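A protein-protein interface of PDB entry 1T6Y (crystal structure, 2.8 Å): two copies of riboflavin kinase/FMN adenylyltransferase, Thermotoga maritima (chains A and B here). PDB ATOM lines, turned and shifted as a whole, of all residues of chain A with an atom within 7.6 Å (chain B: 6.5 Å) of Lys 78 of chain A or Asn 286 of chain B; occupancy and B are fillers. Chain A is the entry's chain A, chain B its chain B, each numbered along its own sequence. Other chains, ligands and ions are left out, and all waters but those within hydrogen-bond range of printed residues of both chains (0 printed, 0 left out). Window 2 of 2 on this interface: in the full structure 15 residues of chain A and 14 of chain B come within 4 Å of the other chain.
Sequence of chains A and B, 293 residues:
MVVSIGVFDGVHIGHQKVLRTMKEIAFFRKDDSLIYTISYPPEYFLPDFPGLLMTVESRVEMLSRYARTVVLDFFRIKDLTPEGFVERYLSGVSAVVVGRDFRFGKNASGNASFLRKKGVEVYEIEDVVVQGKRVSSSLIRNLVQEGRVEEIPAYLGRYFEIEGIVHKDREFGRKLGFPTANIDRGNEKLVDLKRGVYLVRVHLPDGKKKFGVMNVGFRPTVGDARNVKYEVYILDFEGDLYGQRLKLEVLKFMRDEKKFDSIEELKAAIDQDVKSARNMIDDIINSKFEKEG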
ATOM      1  N   PHE A  45      -5.115  -1.063 -24.651  1.00  0.00           N
ATOM      2  CA  PHE A  45      -5.737  -0.141 -25.582  1.00  0.00           C
ATOM      3  C   PHE A  45      -6.687   0.811 -24.876  1.00  0.00           C
ATOM      4  O   PHE A  45      -7.899   0.806 -25.085  1.00  0.00           O
ATOM      5  CB  PHE A  45      -6.439  -0.928 -26.686  1.00  0.00           C
ATOM      6  CG  PHE A  45      -5.507  -1.819 -27.439  1.00  0.00           C
ATOM      7  CD1 PHE A  45      -4.345  -1.299 -27.997  1.00  0.00           C
ATOM      8  CD2 PHE A  45      -5.731  -3.182 -27.513  1.00  0.00           C
ATOM      9  CE1 PHE A  45      -3.417  -2.118 -28.607  1.00  0.00           C
ATOM     10  CE2 PHE A  45      -4.812  -3.999 -28.117  1.00  0.00           C
ATOM     11  CZ  PHE A  45      -3.646  -3.463 -28.666  1.00  0.00           C
ATOM     12  N   ASP A  73      -1.605 -13.089 -31.309  1.00  0.00           N
ATOM     13  CA  ASP A  73      -1.826 -11.671 -31.598  1.00  0.00           C
ATOM     14  C   ASP A  73      -3.224 -11.170 -31.281  1.00  0.00           C
ATOM     15  O   ASP A  73      -4.213 -11.613 -31.875  1.00  0.00           O
ATOM     16  CB  ASP A  73      -1.530 -11.347 -33.054  1.00  0.00           C
ATOM     17  CG  ASP A  73      -1.665  -9.874 -33.342  1.00  0.00           C
ATOM     18  OD1 ASP A  73      -0.760  -9.114 -32.943  1.00  0.00           O
ATOM     19  OD2 ASP A  73      -2.682  -9.478 -33.945  1.00  0.00           O
ATOM     20  N   PHE A  74      -3.277 -10.218 -30.352  1.00  0.00           N
ATOM     21  CA  PHE A  74      -4.526  -9.623 -29.895  1.00  0.00           C
ATOM     22  C   PHE A  74      -5.451  -9.148 -31.006  1.00  0.00           C
ATOM     23  O   PHE A  74      -6.672  -9.215 -30.887  1.00  0.00           O
ATOM     24  CB  PHE A  74      -4.249  -8.431 -28.969  1.00  0.00           C
ATOM     25  CG  PHE A  74      -5.489  -7.883 -28.334  1.00  0.00           C
ATOM     26  CD1 PHE A  74      -6.147  -8.604 -27.335  1.00  0.00           C
ATOM     27  CD2 PHE A  74      -6.055  -6.700 -28.789  1.00  0.00           C
ATOM     28  CE1 PHE A  74      -7.364  -8.155 -26.802  1.00  0.00           C
ATOM     29  CE2 PHE A  74      -7.271  -6.236 -28.265  1.00  0.00           C
ATOM     30  CZ  PHE A  74      -7.929  -6.969 -27.269  1.00  0.00           C
ATOM     31  N   PHE A  75      -4.871  -8.642 -32.081  1.00  0.00           N
ATOM     32  CA  PHE A  75      -5.677  -8.145 -33.176  1.00  0.00           C
ATOM     33  C   PHE A  75      -6.393  -9.307 -33.821  1.00  0.00           C
ATOM     34  O   PHE A  75      -7.616  -9.276 -34.012  1.00  0.00           O
ATOM     35  CB  PHE A  75      -4.769  -7.438 -34.169  1.00  0.00           C
ATOM     36  CG  PHE A  75      -4.104  -6.208 -33.607  1.00  0.00           C
ATOM     37  CD1 PHE A  75      -4.812  -5.009 -33.489  1.00  0.00           C
ATOM     38  CD2 PHE A  75      -2.773  -6.245 -33.203  1.00  0.00           C
ATOM     39  CE1 PHE A  75      -4.203  -3.871 -32.984  1.00  0.00           C
ATOM     40  CE2 PHE A  75      -2.154  -5.104 -32.694  1.00  0.00           C
ATOM     41  CZ  PHE A  75      -2.869  -3.918 -32.585  1.00  0.00           C
ATOM     42  N   ARG A  76      -5.619 -10.347 -34.119  1.00  0.00           N
ATOM     43  CA  ARG A  76      -6.126 -11.567 -34.743  1.00  0.00           C
ATOM     44  C   ARG A  76      -7.180 -12.357 -33.962  1.00  0.00           C
ATOM     45  O   ARG A  76      -7.944 -13.102 -34.564  1.00  0.00           O
ATOM     46  CB  ARG A  76      -4.959 -12.503 -35.066  1.00  0.00           C
ATOM     47  CG  ARG A  76      -4.240 -12.184 -36.360  1.00  0.00           C
ATOM     48  CD  ARG A  76      -2.772 -11.968 -36.156  1.00  0.00           C
ATOM     49  NE  ARG A  76      -2.046 -13.187 -35.841  1.00  0.00           N
ATOM     50  CZ  ARG A  76      -0.720 -13.295 -35.960  1.00  0.00           C
ATOM     51  NH1 ARG A  76      -0.004 -12.258 -36.388  1.00  0.00           N
ATOM     52  NH2 ARG A  76      -0.098 -14.430 -35.658  1.00  0.00           N
ATOM     53  N   ILE A  77      -7.237 -12.203 -32.640  1.00  0.00           N
ATOM     54  CA  ILE A  77      -8.202 -12.972 -31.834  1.00  0.00           C
ATOM     55  C   ILE A  77      -9.268 -12.185 -31.056  1.00  0.00           C
ATOM     56  O   ILE A  77     -10.143 -12.788 -30.449  1.00  0.00           O
ATOM     57  CB  ILE A  77      -7.449 -13.871 -30.800  1.00  0.00           C
ATOM     58  CG1 ILE A  77      -7.234 -13.087 -29.491  1.00  0.00           C
ATOM     59  CG2 ILE A  77      -6.101 -14.356 -31.402  1.00  0.00           C
ATOM     60  CD1 ILE A  77      -6.193 -13.663 -28.567  1.00  0.00           C
ATOM     61  N   LYS A  78      -9.187 -10.854 -31.075  1.00  0.00           N
ATOM     62  CA  LYS A  78     -10.108  -9.991 -30.332  1.00  0.00           C
ATOM     63  C   LYS A  78     -11.579 -10.117 -30.681  1.00  0.00           C
ATOM     64  O   LYS A  78     -12.428  -9.645 -29.931  1.00  0.00           O
ATOM     65  CB  LYS A  78      -9.693  -8.515 -30.471  1.00  0.00           C
ATOM     66  CG  LYS A  78      -9.817  -7.935 -31.887  1.00  0.00           C
ATOM     67  CD  LYS A  78      -9.569  -6.411 -31.942  1.00  0.00           C
ATOM     68  CE  LYS A  78      -8.093  -6.040 -31.697  1.00  0.00           C
ATOM     69  NZ  LYS A  78      -7.797  -4.569 -31.775  1.00  0.00           N
ATOM     70  N   ASP A  79     -11.896 -10.753 -31.805  1.00  0.00           N
ATOM     71  CA  ASP A  79     -13.295 -10.882 -32.202  1.00  0.00           C
ATOM     72  C   ASP A  79     -13.794 -12.325 -32.292  1.00  0.00           C
ATOM     73  O   ASP A  79     -14.989 -12.576 -32.516  1.00  0.00           O
ATOM     74  CB  ASP A  79     -13.520 -10.155 -33.528  1.00  0.00           C
ATOM     75  CG  ASP A  79     -13.281  -8.664 -33.412  1.00  0.00           C
ATOM     76  OD1 ASP A  79     -13.975  -8.010 -32.607  1.00  0.00           O
ATOM     77  OD2 ASP A  79     -12.395  -8.145 -34.121  1.00  0.00           O
ATOM     78  N   LEU A  80     -12.882 -13.268 -32.088  1.00  0.00           N
ATOM     79  CA  LEU A  80     -13.238 -14.676 -32.137  1.00  0.00           C
ATOM     80  C   LEU A  80     -14.141 -15.060 -30.982  1.00  0.00           C
ATOM     81  O   LEU A  80     -13.965 -14.594 -29.856  1.00  0.00           O
ATOM     82  CB  LEU A  80     -11.980 -15.527 -32.110  1.00  0.00           C
ATOM     83  CG  LEU A  80     -11.058 -15.083 -33.242  1.00  0.00           C
ATOM     84  CD1 LEU A  80      -9.749 -15.865 -33.241  1.00  0.00           C
ATOM     85  CD2 LEU A  80     -11.805 -15.256 -34.552  1.00  0.00           C
ATOM     86  N   THR A  81     -15.121 -15.903 -31.278  1.00  0.00           N
ATOM     87  CA  THR A  81     -16.053 -16.373 -30.268  1.00  0.00           C
ATOM     88  C   THR A  81     -15.410 -17.567 -29.577  1.00  0.00           C
ATOM     89  O   THR A  81     -14.420 -18.111 -30.068  1.00  0.00           O
ATOM     90  CB  THR A  81     -17.364 -16.824 -30.913  1.00  0.00           C
ATOM     91  OG1 THR A  81     -17.104 -17.932 -31.784  1.00  0.00           O
ATOM     92  CG2 THR A  81     -17.967 -15.696 -31.716  1.00  0.00           C
ATOM     93  N   PHE A  85     -12.626 -19.616 -31.093  1.00  0.00           N
ATOM     94  CA  PHE A  85     -11.304 -19.734 -30.489  1.00  0.00           C
ATOM     95  C   PHE A  85     -10.827 -21.180 -30.419  1.00  0.00           C
ATOM     96  O   PHE A  85      -9.735 -21.497 -30.895  1.00  0.00           O
ATOM     97  CB  PHE A  85     -11.306 -19.127 -29.085  1.00  0.00           C
ATOM     98  CG  PHE A  85      -9.953 -19.055 -28.464  1.00  0.00           C
ATOM     99  CD1 PHE A  85      -9.046 -18.083 -28.864  1.00  0.00           C
ATOM    100  CD2 PHE A  85      -9.570 -19.982 -27.511  1.00  0.00           C
ATOM    101  CE1 PHE A  85      -7.751 -18.038 -28.313  1.00  0.00           C
ATOM    102  CE2 PHE A  85      -8.298 -19.965 -26.953  1.00  0.00           C
ATOM    103  CZ  PHE A  85      -7.378 -18.991 -27.350  1.00  0.00           C
ATOM    104  N   TYR A  89      -7.620 -22.406 -32.364  1.00  0.00           N
ATOM    105  CA  TYR A  89      -6.441 -22.565 -31.500  1.00  0.00           C
ATOM    106  C   TYR A  89      -6.362 -23.740 -30.537  1.00  0.00           C
ATOM    107  O   TYR A  89      -5.285 -24.007 -29.988  1.00  0.00           O
ATOM    108  CB  TYR A  89      -6.214 -21.292 -30.662  1.00  0.00           C
ATOM    109  CG  TYR A  89      -6.015 -20.035 -31.465  1.00  0.00           C
ATOM    110  CD1 TYR A  89      -4.803 -19.766 -32.084  1.00  0.00           C
ATOM    111  CD2 TYR A  89      -7.071 -19.148 -31.663  1.00  0.00           C
ATOM    112  CE1 TYR A  89      -4.654 -18.651 -32.889  1.00  0.00           C
ATOM    113  CE2 TYR A  89      -6.930 -18.041 -32.459  1.00  0.00           C
ATOM    114  CZ  TYR A  89      -5.725 -17.799 -33.075  1.00  0.00           C
ATOM    115  OH  TYR A  89      -5.616 -16.719 -33.919  1.00  0.00           O
ATOM    116  N   GLY A 105     -12.551 -14.672 -25.618  1.00  0.00           N
ATOM    117  CA  GLY A 105     -13.493 -14.527 -26.718  1.00  0.00           C
ATOM    118  C   GLY A 105     -14.274 -13.226 -26.654  1.00  0.00           C
ATOM    119  O   GLY A 105     -14.688 -12.819 -25.572  1.00  0.00           O
ATOM    120  N   LYS A 106     -14.472 -12.573 -27.799  1.00  0.00           N
ATOM    121  CA  LYS A 106     -15.219 -11.314 -27.855  1.00  0.00           C
ATOM    122  C   LYS A 106     -16.299 -11.266 -26.773  1.00  0.00           C
ATOM    123  O   LYS A 106     -17.282 -12.003 -26.841  1.00  0.00           O
ATOM    124  CB  LYS A 106     -15.873 -11.160 -29.225  1.00  0.00           C
ATOM    125  CG  LYS A 106     -16.733  -9.920 -29.374  1.00  0.00           C
ATOM    126  CD  LYS A 106     -17.425  -9.894 -30.737  1.00  0.00           C
ATOM    127  CE  LYS A 106     -16.414  -9.864 -31.886  1.00  0.00           C
ATOM    128  NZ  LYS A 106     -17.042  -9.932 -33.244  1.00  0.00           N
ATOM    129  N   ASN A 107     -16.104 -10.398 -25.781  1.00  0.00           N
ATOM    130  CA  ASN A 107     -17.031 -10.239 -24.654  1.00  0.00           C
ATOM    131  C   ASN A 107     -16.795 -11.277 -23.566  1.00  0.00           C
ATOM    132  O   ASN A 107     -17.722 -11.658 -22.844  1.00  0.00           O
ATOM    133  CB  ASN A 107     -18.492 -10.338 -25.102  1.00  0.00           C
ATOM    134  CG  ASN A 107     -18.852  -9.310 -26.144  1.00  0.00           C
ATOM    135  OD1 ASN A 107     -18.379  -8.169 -26.103  1.00  0.00           O
ATOM    136  ND2 ASN A 107     -19.712  -9.701 -27.081  1.00  0.00           N
ATOM    137  N   ALA A 108     -15.553 -11.736 -23.453  1.00  0.00           N
ATOM    138  CA  ALA A 108     -15.201 -12.730 -22.449  1.00  0.00           C
ATOM    139  C   ALA A 108     -16.244 -13.840 -22.508  1.00  0.00           C
ATOM    140  O   ALA A 108     -16.534 -14.517 -21.530  1.00  0.00           O
ATOM    141  CB  ALA A 108     -15.181 -12.078 -21.080  1.00  0.00           C
ATOM    142  N   ILE B 281     -18.506  -1.802 -23.904  1.00  0.00           N
ATOM    143  CA  ILE B 281     -17.103  -2.013 -23.579  1.00  0.00           C
ATOM    144  C   ILE B 281     -16.337  -2.398 -24.836  1.00  0.00           C
ATOM    145  O   ILE B 281     -15.224  -1.915 -25.074  1.00  0.00           O
ATOM    146  CB  ILE B 281     -16.923  -3.143 -22.535  1.00  0.00           C
ATOM    147  CG1 ILE B 281     -17.859  -2.910 -21.350  1.00  0.00           C
ATOM    148  CG2 ILE B 281     -15.477  -3.208 -22.078  1.00  0.00           C
ATOM    149  CD1 ILE B 281     -17.466  -3.656 -20.093  1.00  0.00           C
ATOM    150  N   ASP B 282     -16.923  -3.276 -25.646  1.00  0.00           N
ATOM    151  CA  ASP B 282     -16.247  -3.686 -26.869  1.00  0.00           C
ATOM    152  C   ASP B 282     -16.076  -2.441 -27.743  1.00  0.00           C
ATOM    153  O   ASP B 282     -15.065  -2.282 -28.436  1.00  0.00           O
ATOM    154  CB  ASP B 282     -17.045  -4.771 -27.602  1.00  0.00           C
ATOM    155  CG  ASP B 282     -16.143  -5.759 -28.341  1.00  0.00           C
ATOM    156  OD1 ASP B 282     -15.391  -6.506 -27.669  1.00  0.00           O
ATOM    157  OD2 ASP B 282     -16.179  -5.784 -29.590  1.00  0.00           O
ATOM    158  N   ASP B 283     -17.070  -1.555 -27.684  1.00  0.00           N
ATOM    159  CA  ASP B 283     -17.044  -0.302 -28.433  1.00  0.00           C
ATOM    160  C   ASP B 283     -15.848   0.536 -27.979  1.00  0.00           C
ATOM    161  O   ASP B 283     -15.022   0.962 -28.791  1.00  0.00           O
ATOM    162  CB  ASP B 283     -18.338   0.483 -28.194  1.00  0.00           C
ATOM    163  CG  ASP B 283     -19.539  -0.137 -28.889  1.00  0.00           C
ATOM    164  OD1 ASP B 283     -19.759  -1.361 -28.731  1.00  0.00           O
ATOM    165  OD2 ASP B 283     -20.268   0.602 -29.591  1.00  0.00           O
ATOM    166  N   ILE B 284     -15.755   0.743 -26.671  1.00  0.00           N
ATOM    167  CA  ILE B 284     -14.679   1.529 -26.088  1.00  0.00           C
ATOM    168  C   ILE B 284     -13.269   1.054 -26.454  1.00  0.00           C
ATOM    169  O   ILE B 284     -12.289   1.761 -26.206  1.00  0.00           O
ATOM    170  CB  ILE B 284     -14.810   1.561 -24.549  1.00  0.00           C
ATOM    171  CG1 ILE B 284     -16.197   2.082 -24.167  1.00  0.00           C
ATOM    172  CG2 ILE B 284     -13.710   2.424 -23.934  1.00  0.00           C
ATOM    173  CD1 ILE B 284     -16.449   2.108 -22.669  1.00  0.00           C
ATOM    174  N   ILE B 285     -13.152  -0.129 -27.046  1.00  0.00           N
ATOM    175  CA  ILE B 285     -11.831  -0.626 -27.409  1.00  0.00           C
ATOM    176  C   ILE B 285     -11.649  -0.761 -28.915  1.00  0.00           C
ATOM    177  O   ILE B 285     -10.554  -0.539 -29.436  1.00  0.00           O
ATOM    178  CB  ILE B 285     -11.551  -1.969 -26.724  1.00  0.00           C
ATOM    179  CG1 ILE B 285     -11.703  -1.797 -25.210  1.00  0.00           C
ATOM    180  CG2 ILE B 285     -10.142  -2.449 -27.064  1.00  0.00           C
ATOM    181  CD1 ILE B 285     -11.561  -3.068 -24.422  1.00  0.00           C
ATOM    182  N   ASN B 286     -12.717  -1.131 -29.618  1.00  0.00           N
ATOM    183  CA  ASN B 286     -12.640  -1.253 -31.072  1.00  0.00           C
ATOM    184  C   ASN B 286     -12.545   0.159 -31.648  1.00  0.00           C
ATOM    185  O   ASN B 286     -12.508   0.346 -32.868  1.00  0.00           O
ATOM    186  CB  ASN B 286     -13.885  -1.956 -31.646  1.00  0.00           C
ATOM    187  CG  ASN B 286     -13.771  -3.480 -31.631  1.00  0.00           C
ATOM    188  OD1 ASN B 286     -12.747  -4.046 -32.019  1.00  0.00           O
ATOM    189  ND2 ASN B 286     -14.837  -4.146 -31.204  1.00  0.00           N
ATOM    190  N   SER B 287     -12.503   1.152 -30.762  1.00  0.00           N
ATOM    191  CA  SER B 287     -12.422   2.543 -31.190  1.00  0.00           C
ATOM    192  C   SER B 287     -11.057   3.173 -30.947  1.00  0.00           C
ATOM    193  O   SER B 287     -10.962   4.353 -30.637  1.00  0.00           O
ATOM    194  CB  SER B 287     -13.503   3.373 -30.492  1.00  0.00           C
ATOM    195  OG  SER B 287     -13.293   3.400 -29.095  1.00  0.00           O
ATOM    196  N   LYS B 288      -9.997   2.389 -31.097  1.00  0.00           N
ATOM    197  CA  LYS B 288      -8.643   2.899 -30.903  1.00  0.00           C
ATOM    198  C   LYS B 288      -7.802   2.698 -32.168  1.00  0.00           C
ATOM    199  O   LYS B 288      -6.651   3.138 -32.238  1.00  0.00           O
ATOM    200  CB  LYS B 288      -7.977   2.197 -29.704  1.00  0.00           C
ATOM    201  CG  LYS B 288      -8.190   2.877 -28.339  1.00  0.00           C
ATOM    202  CD  LYS B 288      -9.664   3.096 -28.004  1.00  0.00           C
ATOM    203  CE  LYS B 288      -9.843   3.673 -26.599  1.00  0.00           C
ATOM    204  NZ  LYS B 288      -8.986   4.874 -26.325  1.00  0.00           N
ATOM    205  N   PHE B 289      -8.395   2.044 -33.168  1.00  0.00           N
ATOM    206  CA  PHE B 289      -7.726   1.758 -34.440  1.00  0.00           C
ATOM    207  C   PHE B 289      -8.649   2.032 -35.625  1.00  0.00           C
ATOM    208  O   PHE B 289      -9.833   2.323 -35.449  1.00  0.00           O
ATOM    209  CB  PHE B 289      -7.262   0.294 -34.474  1.00  0.00           C
ATOM    210  CG  PHE B 289      -7.604  -0.487 -33.224  1.00  0.00           C
ATOM    211  CD1 PHE B 289      -8.899  -0.959 -33.005  1.00  0.00           C
ATOM    212  CD2 PHE B 289      -6.633  -0.722 -32.249  1.00  0.00           C
ATOM    213  CE1 PHE B 289      -9.220  -1.650 -31.834  1.00  0.00           C
ATOM    214  CE2 PHE B 289      -6.946  -1.410 -31.079  1.00  0.00           C
ATOM    215  CZ  PHE B 289      -8.242  -1.874 -30.872  1.00  0.00           C
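No position is printed for both chains.
Printed residues of chain A within 4 Å of Lys 288 of chain B: Phe 45 (3.8 Å). Printed residues of chain A within 4 Å of Phe 289 of chain B: Phe 45 and Lys 78. Of the printed residues of chain A, Asp 282 of chain B touches Asn 107 (3.8 Å). Asp 283 of chain B touches none of the printed residues of chain A. Ile 77 of chain A touches none of the printed residues of chain B. The nearest residue of chain B that does not touch Lys 78 of chain A is Asp 282 of chain B (4.9 Å). The nearest printed residue of chain B that does not touch Asn 107 of chain A is Ile 281 of chain B (6.3 Å).
Among the printed residues, merely in contact across the chains: Lys 78 of chain A with Phe 289 of chain B, Asn 107 of chain A with Asp 282 of chain B, Phe 45 of chain A with Lys 288 of chain B, Phe 45 of chain A with Phe 289 of chain B and Lys 78 of chain A with Asn 286 of chain B.
ND2 of Asn 286 of chain B sits at hydrogen-bond distance from OD2 of Asp 282 of chain B (2.7 Å).
Hydrophobic or aromatic side chains of chain B that line the printed part of chain A: Phe 289. Of the 16 printed residues of chain A, 3 touch a printed residue of chain B. Hydrophobic or aromatic side chains of chain A within 4 Å of the printed part of chain B: Phe 45. Among the printed residues, 5 pairs touch across the chains. Among the printed residues, no Asp or Glu carboxylate lies within 4 Å of a Lys or Arg side-chain nitrogen of the other chain.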
